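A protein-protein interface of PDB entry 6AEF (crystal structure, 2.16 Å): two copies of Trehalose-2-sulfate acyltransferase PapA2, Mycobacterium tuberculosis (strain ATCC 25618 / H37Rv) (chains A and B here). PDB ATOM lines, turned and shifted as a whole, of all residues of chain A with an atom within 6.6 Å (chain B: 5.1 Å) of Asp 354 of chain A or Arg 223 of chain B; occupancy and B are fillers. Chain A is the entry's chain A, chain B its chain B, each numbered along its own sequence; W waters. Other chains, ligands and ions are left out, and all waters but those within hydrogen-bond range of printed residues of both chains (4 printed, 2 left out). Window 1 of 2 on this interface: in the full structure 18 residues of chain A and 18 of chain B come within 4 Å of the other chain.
Among the printed residues, pairs that only touch across the chains: Arg 223 of chain A with Arg 223 of chain B (3.6 Å), Arg 312 of chain A with Ala 216 of chain B (3.6 Å), Ser 351 of chain A with Ser 221 of chain B (3.6 Å) and Asp 354 of chain A with Leu 217 of chain B (3.3 Å).
OD1 of Asp 354 of chain B lies within salt-bridge range of NH2 of Arg 223 of chain A (2.6 Å). NH2 of Arg 223 of chain B lies within salt-bridge range of OD1 of Asp 354 of chain A.
Water W2 lies within hydrogen-bond range of OD2 of Asp 354 of chain A (2.7 Å), N of Arg 223 of chain B (3.0 Å) and N of Ala 222 of chain B (3.1 Å). Water W1 lies within hydrogen-bond range of OD1 of Asp 354 of chain B and NH2 of Arg 223 of chain A. Water W4 lies within hydrogen-bond range of OD2 of Asp 354 of chain B (2.8 Å), N of Arg 223 of chain A (2.9 Å) and N of Ala 222 of chain A (3.1 Å). Water W3 lies within hydrogen-bond range of the side-chain carboxylate of Asp 354 of chain A (2.8 Å), the guanidinium group of Arg 312 of chain A (3.1 Å) and the guanidinium group of Arg 223 of chain B (3.4 Å).
The backbone carbonyl oxygen (O) of Asp 354 of chain A lies within hydrogen-bond range of the side-chain hydroxyl (OG1) of Thr 357 of chain A. The side-chain hydroxyl (OG1) of Thr 357 of chain B is in hydrogen-bond range of the guanidinium group (NH1) of Arg 223 of chain B, 3.0 Å away. The guanidinium group (NH1) of Arg 223 of chain A lies within salt-bridge range of the side-chain carboxylate (OD1) of Asp 354 of chain A (3.8 Å). NH1 of Arg 223 of chain B lies within salt-bridge range of OD1 of Asp 354 of chain B, 3.8 Å away. The backbone carbonyl oxygen of Lys 353 of chain A sits at hydrogen-bond distance from the guanidinium group of Arg 312 of chain A. The side-chain hydroxyl (OG1) of Thr 357 of chain B sits at hydrogen-bond distance from the backbone carbonyl oxygen (O) of Asp 354 of chain B (3.4 Å).
Arg 223 of chain A touches its own counterpart, Arg 223 of chain B. Arg 223 of chain A touches Asp 354 of chain B, and with the chains exchanged Asp 354 of chain A touches Arg 223 of chain B. 6 positions are printed for both chains. Of the 6 pairs that touch across the chains among the printed residues, 3 have their exchanged pair printed and touching as well.
Of the 13 printed residues of chain B, 5 touch a printed residue of chain A. Hydrophobic or aromatic side chains of chain B that line the printed part of chain A: Ala 216 and Leu 217. Among the printed residues, Asp or Glu carboxylates within 4 Å of a Lys or Arg side-chain nitrogen of the other chain: Arg 223 of chain A with Asp 354 of chain B (2.6 Å) and Asp 354 of chain A with Arg 223 of chain B (2.9 Å).
Asp 354 of chain A touches just these residues of chain B: Leu 217 (3.3 Å) and Arg 223 (2.9 Å). Arg 223 of chain B touches two residues of chain A. Printed residues of chain B within 4 Å of Arg 223 of chain A: Arg 223 and Asp 354. Of the printed residues of chain A, Ala 216 of chain B touches Arg 312 (3.6 Å). Trp 227 of chain B touches none of the printed residues of chain A. The nearest residue of chain B that does not touch Asp 354 of chain A is Ser 221 of chain B (4.2 Å). The nearest printed residue of chain A that does not touch Ala 216 of chain B is Lys 353 of chain A (4.2 Å).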
ATOM      1  N   ALA A 222     -23.951  35.515  14.919  1.00  0.00           N
ATOM      2  CA  ALA A 222     -24.005  34.499  15.969  1.00  0.00           C
ATOM      3  C   ALA A 222     -23.249  33.230  15.577  1.00  0.00           C
ATOM      4  O   ALA A 222     -22.531  32.649  16.399  1.00  0.00           O
ATOM      5  CB  ALA A 222     -25.458  34.167  16.303  1.00  0.00           C
ATOM      6  N   ARG A 223     -23.419  32.765  14.340  1.00  0.00           N
ATOM      7  CA  ARG A 223     -22.757  31.527  13.934  1.00  0.00           C
ATOM      8  C   ARG A 223     -21.240  31.691  13.904  1.00  0.00           C
ATOM      9  O   ARG A 223     -20.498  30.800  14.352  1.00  0.00           O
ATOM     10  CB  ARG A 223     -23.292  31.080  12.574  1.00  0.00           C
ATOM     11  CG  ARG A 223     -24.752  30.635  12.608  1.00  0.00           C
ATOM     12  CD  ARG A 223     -25.146  29.851  11.349  1.00  0.00           C
ATOM     13  NE  ARG A 223     -25.345  30.721  10.203  1.00  0.00           N
ATOM     14  CZ  ARG A 223     -25.579  30.298   8.967  1.00  0.00           C
ATOM     15  NH1 ARG A 223     -25.643  28.998   8.701  1.00  0.00           N
ATOM     16  NH2 ARG A 223     -25.755  31.177   7.989  1.00  0.00           N
ATOM     17  N   ARG A 312     -29.119  19.958   1.158  1.00  0.00           N
ATOM     18  CA  ARG A 312     -30.418  20.075   1.816  1.00  0.00           C
ATOM     19  C   ARG A 312     -31.617  19.992   0.874  1.00  0.00           C
ATOM     20  O   ARG A 312     -32.579  19.279   1.174  1.00  0.00           O
ATOM     21  CB  ARG A 312     -30.467  21.375   2.613  1.00  0.00           C
ATOM     22  CG  ARG A 312     -29.816  21.210   3.967  1.00  0.00           C
ATOM     23  CD  ARG A 312     -29.667  22.505   4.680  1.00  0.00           C
ATOM     24  NE  ARG A 312     -28.827  22.359   5.863  1.00  0.00           N
ATOM     25  CZ  ARG A 312     -28.500  23.363   6.666  1.00  0.00           C
ATOM     26  NH1 ARG A 312     -28.946  24.583   6.414  1.00  0.00           N
ATOM     27  NH2 ARG A 312     -27.730  23.146   7.721  1.00  0.00           N
ATOM     28  N   VAL A 327     -18.792  20.276  11.803  1.00  0.00           N
ATOM     29  CA  VAL A 327     -19.616  20.557  12.976  1.00  0.00           C
ATOM     30  C   VAL A 327     -18.711  20.558  14.205  1.00  0.00           C
ATOM     31  O   VAL A 327     -17.973  19.584  14.417  1.00  0.00           O
ATOM     32  CB  VAL A 327     -20.746  19.522  13.140  1.00  0.00           C
ATOM     33  CG1 VAL A 327     -21.638  19.872  14.325  1.00  0.00           C
ATOM     34  CG2 VAL A 327     -21.565  19.407  11.852  1.00  0.00           C
ATOM     35  N   PHE A 349     -24.305  17.859  18.410  1.00  0.00           N
ATOM     36  CA  PHE A 349     -24.348  17.415  17.021  1.00  0.00           C
ATOM     37  C   PHE A 349     -25.511  18.070  16.274  1.00  0.00           C
ATOM     38  O   PHE A 349     -25.320  18.763  15.262  1.00  0.00           O
ATOM     39  CB  PHE A 349     -24.455  15.885  17.014  1.00  0.00           C
ATOM     40  CG  PHE A 349     -24.378  15.252  15.651  1.00  0.00           C
ATOM     41  CD1 PHE A 349     -23.205  15.283  14.916  1.00  0.00           C
ATOM     42  CD2 PHE A 349     -25.465  14.564  15.136  1.00  0.00           C
ATOM     43  CE1 PHE A 349     -23.129  14.669  13.671  1.00  0.00           C
ATOM     44  CE2 PHE A 349     -25.393  13.946  13.892  1.00  0.00           C
ATOM     45  CZ  PHE A 349     -24.224  13.999  13.162  1.00  0.00           C
ATOM     46  N   ASP A 350     -26.726  17.899  16.799  1.00  0.00           N
ATOM     47  CA  ASP A 350     -27.914  18.383  16.108  1.00  0.00           C
ATOM     48  C   ASP A 350     -27.886  19.900  15.963  1.00  0.00           C
ATOM     49  O   ASP A 350     -27.988  20.428  14.851  1.00  0.00           O
ATOM     50  CB  ASP A 350     -29.170  17.929  16.856  1.00  0.00           C
ATOM     51  CG  ASP A 350     -29.343  16.416  16.850  1.00  0.00           C
ATOM     52  OD1 ASP A 350     -28.775  15.745  15.959  1.00  0.00           O
ATOM     53  OD2 ASP A 350     -30.044  15.898  17.744  1.00  0.00           O
ATOM     54  N   SER A 351     -27.716  20.620  17.072  1.00  0.00           N
ATOM     55  CA  SER A 351     -27.683  22.077  17.008  1.00  0.00           C
ATOM     56  C   SER A 351     -26.494  22.579  16.206  1.00  0.00           C
ATOM     57  O   SER A 351     -26.534  23.705  15.700  1.00  0.00           O
ATOM     58  CB  SER A 351     -27.647  22.678  18.415  1.00  0.00           C
ATOM     59  OG  SER A 351     -26.401  22.445  19.047  1.00  0.00           O
ATOM     60  N   GLY A 352     -25.433  21.774  16.096  1.00  0.00           N
ATOM     61  CA  GLY A 352     -24.284  22.148  15.294  1.00  0.00           C
ATOM     62  C   GLY A 352     -24.468  21.952  13.805  1.00  0.00           C
ATOM     63  O   GLY A 352     -23.671  22.474  13.024  1.00  0.00           O
ATOM     64  N   LYS A 353     -25.486  21.201  13.385  1.00  0.00           N
ATOM     65  CA  LYS A 353     -25.743  21.089  11.947  1.00  0.00           C
ATOM     66  C   LYS A 353     -25.848  22.466  11.278  1.00  0.00           C
ATOM     67  O   LYS A 353     -25.348  22.665  10.163  1.00  0.00           O
ATOM     68  CB  LYS A 353     -27.017  20.284  11.693  1.00  0.00           C
ATOM     69  CG  LYS A 353     -26.951  18.822  12.145  1.00  0.00           C
ATOM     70  CD  LYS A 353     -25.731  18.108  11.602  1.00  0.00           C
ATOM     71  CE  LYS A 353     -25.753  16.630  11.935  1.00  0.00           C
ATOM     72  NZ  LYS A 353     -26.825  15.892  11.211  1.00  0.00           N
ATOM     73  N   ASP A 354     -26.495  23.432  11.942  1.00  0.00           N
ATOM     74  CA  ASP A 354     -26.652  24.763  11.358  1.00  0.00           C
ATOM     75  C   ASP A 354     -25.317  25.475  11.163  1.00  0.00           C
ATOM     76  O   ASP A 354     -25.259  26.453  10.410  1.00  0.00           O
ATOM     77  CB  ASP A 354     -27.568  25.626  12.235  1.00  0.00           C
ATOM     78  CG  ASP A 354     -28.042  26.899  11.521  1.00  0.00           C
ATOM     79  OD1 ASP A 354     -28.371  26.819  10.310  1.00  0.00           O
ATOM     80  OD2 ASP A 354     -28.097  27.974  12.174  1.00  0.00           O
ATOM     81  N   LEU A 355     -24.254  25.021  11.828  1.00  0.00           N
ATOM     82  CA  LEU A 355     -22.944  25.649  11.708  1.00  0.00           C
ATOM     83  C   LEU A 355     -22.093  25.050  10.594  1.00  0.00           C
ATOM     84  O   LEU A 355     -21.095  25.665  10.197  1.00  0.00           O
ATOM     85  CB  LEU A 355     -22.180  25.530  13.030  1.00  0.00           C
ATOM     86  CG  LEU A 355     -22.804  26.131  14.294  1.00  0.00           C
ATOM     87  CD1 LEU A 355     -21.925  25.826  15.499  1.00  0.00           C
ATOM     88  CD2 LEU A 355     -23.019  27.629  14.166  1.00  0.00           C
ATOM     89  N   ALA A 356     -22.460  23.872  10.082  1.00  0.00           N
ATOM     90  CA  ALA A 356     -21.634  23.195   9.085  1.00  0.00           C
ATOM     91  C   ALA A 356     -21.591  23.943   7.765  1.00  0.00           C
ATOM     92  O   ALA A 356     -20.669  23.732   6.973  1.00  0.00           O
ATOM     93  CB  ALA A 356     -22.143  21.775   8.844  1.00  0.00           C
ATOM     94  N   THR A 357     -22.563  24.810   7.511  1.00  0.00           N
ATOM     95  CA  THR A 357     -22.589  25.585   6.282  1.00  0.00           C
ATOM     96  C   THR A 357     -21.743  26.847   6.362  1.00  0.00           C
ATOM     97  O   THR A 357     -21.632  27.554   5.357  1.00  0.00           O
ATOM     98  CB  THR A 357     -24.034  25.952   5.940  1.00  0.00           C
ATOM     99  OG1 THR A 357     -24.639  26.569   7.074  1.00  0.00           O
ATOM    100  CG2 THR A 357     -24.828  24.717   5.568  1.00  0.00           C
ATOM    101  N   VAL A 358     -21.137  27.133   7.510  1.00  0.00           N
ATOM    102  CA  VAL A 358     -20.210  28.254   7.654  1.00  0.00           C
ATOM    103  C   VAL A 358     -18.791  27.700   7.543  1.00  0.00           C
ATOM    104  O   VAL A 358     -18.329  27.019   8.474  1.00  0.00           O
ATOM    105  CB  VAL A 358     -20.403  28.987   8.986  1.00  0.00           C
ATOM    106  CG1 VAL A 358     -19.358  30.081   9.126  1.00  0.00           C
ATOM    107  CG2 VAL A 358     -21.800  29.550   9.084  1.00  0.00           C
ATOM    108  N   ALA B 216     -33.367  22.058   9.526  1.00  0.00           N
ATOM    109  CA  ALA B 216     -32.041  21.797  10.060  1.00  0.00           C
ATOM    110  C   ALA B 216     -31.796  22.483  11.396  1.00  0.00           C
ATOM    111  O   ALA B 216     -30.771  22.207  12.030  1.00  0.00           O
ATOM    112  CB  ALA B 216     -30.987  22.247   9.050  1.00  0.00           C
ATOM    113  N   LEU B 217     -32.698  23.359  11.831  1.00  0.00           N
ATOM    114  CA  LEU B 217     -32.545  24.086  13.083  1.00  0.00           C
ATOM    115  C   LEU B 217     -33.182  23.308  14.225  1.00  0.00           C
ATOM    116  O   LEU B 217     -34.217  22.663  14.051  1.00  0.00           O
ATOM    117  CB  LEU B 217     -33.213  25.461  12.987  1.00  0.00           C
ATOM    118  CG  LEU B 217     -32.745  26.410  11.888  1.00  0.00           C
ATOM    119  CD1 LEU B 217     -33.601  27.658  11.882  1.00  0.00           C
ATOM    120  CD2 LEU B 217     -31.285  26.763  12.072  1.00  0.00           C
ATOM    121  N   SER B 221     -29.808  25.505  18.386  1.00  0.00           N
ATOM    122  CA  SER B 221     -29.009  26.164  17.359  1.00  0.00           C
ATOM    123  C   SER B 221     -28.760  27.623  17.740  1.00  0.00           C
ATOM    124  O   SER B 221     -29.627  28.287  18.308  1.00  0.00           O
ATOM    125  CB  SER B 221     -29.722  26.098  16.006  1.00  0.00           C
ATOM    126  OG  SER B 221     -29.948  24.762  15.582  1.00  0.00           O
ATOM    127  N   ALA B 222     -27.570  28.125  17.403  1.00  0.00           N
ATOM    128  CA  ALA B 222     -27.165  29.458  17.840  1.00  0.00           C
ATOM    129  C   ALA B 222     -28.135  30.529  17.356  1.00  0.00           C
ATOM    130  O   ALA B 222     -28.511  31.427  18.115  1.00  0.00           O
ATOM    131  CB  ALA B 222     -25.750  29.761  17.352  1.00  0.00           C
ATOM    132  N   ARG B 223     -28.542  30.467  16.089  1.00  0.00           N
ATOM    133  CA  ARG B 223     -29.420  31.510  15.567  1.00  0.00           C
ATOM    134  C   ARG B 223     -30.772  31.482  16.267  1.00  0.00           C
ATOM    135  O   ARG B 223     -31.348  32.539  16.580  1.00  0.00           O
ATOM    136  CB  ARG B 223     -29.576  31.355  14.056  1.00  0.00           C
ATOM    137  CG  ARG B 223     -28.302  31.663  13.286  1.00  0.00           C
ATOM    138  CD  ARG B 223     -28.596  31.871  11.806  1.00  0.00           C
ATOM    139  NE  ARG B 223     -28.821  30.610  11.109  1.00  0.00           N
ATOM    140  CZ  ARG B 223     -29.216  30.508   9.843  1.00  0.00           C
ATOM    141  NH1 ARG B 223     -29.443  31.599   9.111  1.00  0.00           N
ATOM    142  NH2 ARG B 223     -29.386  29.307   9.308  1.00  0.00           N
ATOM    143  N   VAL B 224     -31.278  30.275  16.539  1.00  0.00           N
ATOM    144  CA  VAL B 224     -32.517  30.141  17.294  1.00  0.00           C
ATOM    145  C   VAL B 224     -32.340  30.687  18.707  1.00  0.00           C
ATOM    146  O   VAL B 224     -33.201  31.418  19.211  1.00  0.00           O
ATOM    147  CB  VAL B 224     -32.989  28.674  17.286  1.00  0.00           C
ATOM    148  CG1 VAL B 224     -34.199  28.477  18.190  1.00  0.00           C
ATOM    149  CG2 VAL B 224     -33.330  28.262  15.878  1.00  0.00           C
ATOM    150  N   ARG B 225     -31.228  30.347  19.370  1.00  0.00           N
ATOM    151  CA  ARG B 225     -31.000  30.879  20.715  1.00  0.00           C
ATOM    152  C   ARG B 225     -30.950  32.400  20.707  1.00  0.00           C
ATOM    153  O   ARG B 225     -31.415  33.051  21.648  1.00  0.00           O
ATOM    154  CB  ARG B 225     -29.709  30.334  21.324  1.00  0.00           C
ATOM    155  CG  ARG B 225     -29.856  28.984  22.026  1.00  0.00           C
ATOM    156  CD  ARG B 225     -28.701  28.730  22.996  1.00  0.00           C
ATOM    157  NE  ARG B 225     -27.629  27.904  22.448  1.00  0.00           N
ATOM    158  CZ  ARG B 225     -27.386  26.636  22.788  1.00  0.00           C
ATOM    159  NH1 ARG B 225     -28.138  26.008  23.682  1.00  0.00           N
ATOM    160  NH2 ARG B 225     -26.373  25.990  22.227  1.00  0.00           N
ATOM    161  N   ARG B 226     -30.392  32.985  19.652  1.00  0.00           N
ATOM    162  CA  ARG B 226     -30.327  34.437  19.584  1.00  0.00           C
ATOM    163  C   ARG B 226     -31.729  35.029  19.492  1.00  0.00           C
ATOM    164  O   ARG B 226     -32.075  35.943  20.248  1.00  0.00           O
ATOM    165  CB  ARG B 226     -29.452  34.859  18.405  1.00  0.00           C
ATOM    166  CG  ARG B 226     -29.193  36.344  18.298  1.00  0.00           C
ATOM    167  CD  ARG B 226     -28.376  36.898  19.465  1.00  0.00           C
ATOM    168  NE  ARG B 226     -28.418  38.358  19.478  1.00  0.00           N
ATOM    169  CZ  ARG B 226     -29.369  39.086  20.060  1.00  0.00           C
ATOM    170  NH1 ARG B 226     -30.372  38.499  20.701  1.00  0.00           N
ATOM    171  NH2 ARG B 226     -29.316  40.410  20.003  1.00  0.00           N
ATOM    172  N   TRP B 227     -32.570  34.493  18.602  1.00  0.00           N
ATOM    173  CA  TRP B 227     -33.964  34.938  18.584  1.00  0.00           C
ATOM    174  C   TRP B 227     -34.623  34.761  19.957  1.00  0.00           C
ATOM    175  O   TRP B 227     -35.360  35.639  20.419  1.00  0.00           O
ATOM    176  CB  TRP B 227     -34.747  34.179  17.522  1.00  0.00           C
ATOM    177  CG  TRP B 227     -34.679  34.795  16.175  1.00  0.00           C
ATOM    178  CD1 TRP B 227     -34.036  34.297  15.092  1.00  0.00           C
ATOM    179  CD2 TRP B 227     -35.272  36.031  15.762  1.00  0.00           C
ATOM    180  NE1 TRP B 227     -34.187  35.142  14.019  1.00  0.00           N
ATOM    181  CE2 TRP B 227     -34.943  36.216  14.407  1.00  0.00           C
ATOM    182  CE3 TRP B 227     -36.050  36.999  16.407  1.00  0.00           C
ATOM    183  CZ2 TRP B 227     -35.364  37.323  13.680  1.00  0.00           C
ATOM    184  CZ3 TRP B 227     -36.464  38.100  15.687  1.00  0.00           C
ATOM    185  CH2 TRP B 227     -36.118  38.258  14.338  1.00  0.00           C
ATOM    186  N   ASP B 354     -27.771  37.564   9.082  1.00  0.00           N
ATOM    187  CA  ASP B 354     -27.779  36.102   9.079  1.00  0.00           C
ATOM    188  C   ASP B 354     -28.991  35.528   9.809  1.00  0.00           C
ATOM    189  O   ASP B 354     -29.324  34.354   9.612  1.00  0.00           O
ATOM    190  CB  ASP B 354     -26.496  35.548   9.716  1.00  0.00           C
ATOM    191  CG  ASP B 354     -26.264  34.066   9.386  1.00  0.00           C
ATOM    192  OD1 ASP B 354     -26.378  33.696   8.200  1.00  0.00           O
ATOM    193  OD2 ASP B 354     -25.945  33.272  10.299  1.00  0.00           O
ATOM    194  N   LEU B 355     -29.658  36.329  10.637  1.00  0.00           N
ATOM    195  CA  LEU B 355     -30.830  35.880  11.372  1.00  0.00           C
ATOM    196  C   LEU B 355     -32.120  36.099  10.601  1.00  0.00           C
ATOM    197  O   LEU B 355     -33.145  35.519  10.971  1.00  0.00           O
ATOM    198  CB  LEU B 355     -30.915  36.607  12.717  1.00  0.00           C
ATOM    199  CG  LEU B 355     -29.734  36.436  13.666  1.00  0.00           C
ATOM    200  CD1 LEU B 355     -29.940  37.306  14.905  1.00  0.00           C
ATOM    201  CD2 LEU B 355     -29.563  34.982  14.064  1.00  0.00           C
ATOM    202  N   THR B 357     -33.097  35.060   7.773  1.00  0.00           N
ATOM    203  CA  THR B 357     -33.568  33.856   7.107  1.00  0.00           C
ATOM    204  C   THR B 357     -34.143  32.827   8.072  1.00  0.00           C
ATOM    205  O   THR B 357     -34.562  31.755   7.630  1.00  0.00           O
ATOM    206  CB  THR B 357     -32.426  33.217   6.319  1.00  0.00           C
ATOM    207  OG1 THR B 357     -31.318  32.997   7.196  1.00  0.00           O
ATOM    208  CG2 THR B 357     -32.001  34.139   5.184  1.00  0.00           C
ATOM    209  N   VAL B 358     -34.126  33.104   9.374  1.00  0.00           N
ATOM    210  CA  VAL B 358     -34.769  32.258  10.375  1.00  0.00           C
ATOM    211  C   VAL B 358     -36.125  32.881  10.699  1.00  0.00           C
ATOM    212  O   VAL B 358     -36.170  33.901  11.409  1.00  0.00           O
ATOM    213  CB  VAL B 358     -33.914  32.128  11.637  1.00  0.00           C
ATOM    214  CG1 VAL B 358     -34.670  31.351  12.710  1.00  0.00           C
ATOM    215  CG2 VAL B 358     -32.593  31.453  11.310  1.00  0.00           C
HETATM  216  O   HOH W   1     -25.758  33.396   5.543  1.00  0.00           O
HETATM  217  O   HOH W   2     -26.809  28.593  14.468  1.00  0.00           O
HETATM  218  O   HOH W   3     -30.485  26.202   8.504  1.00  0.00           O
HETATM  219  O   HOH W   4     -25.698  33.964  12.956  1.00  0.00           O
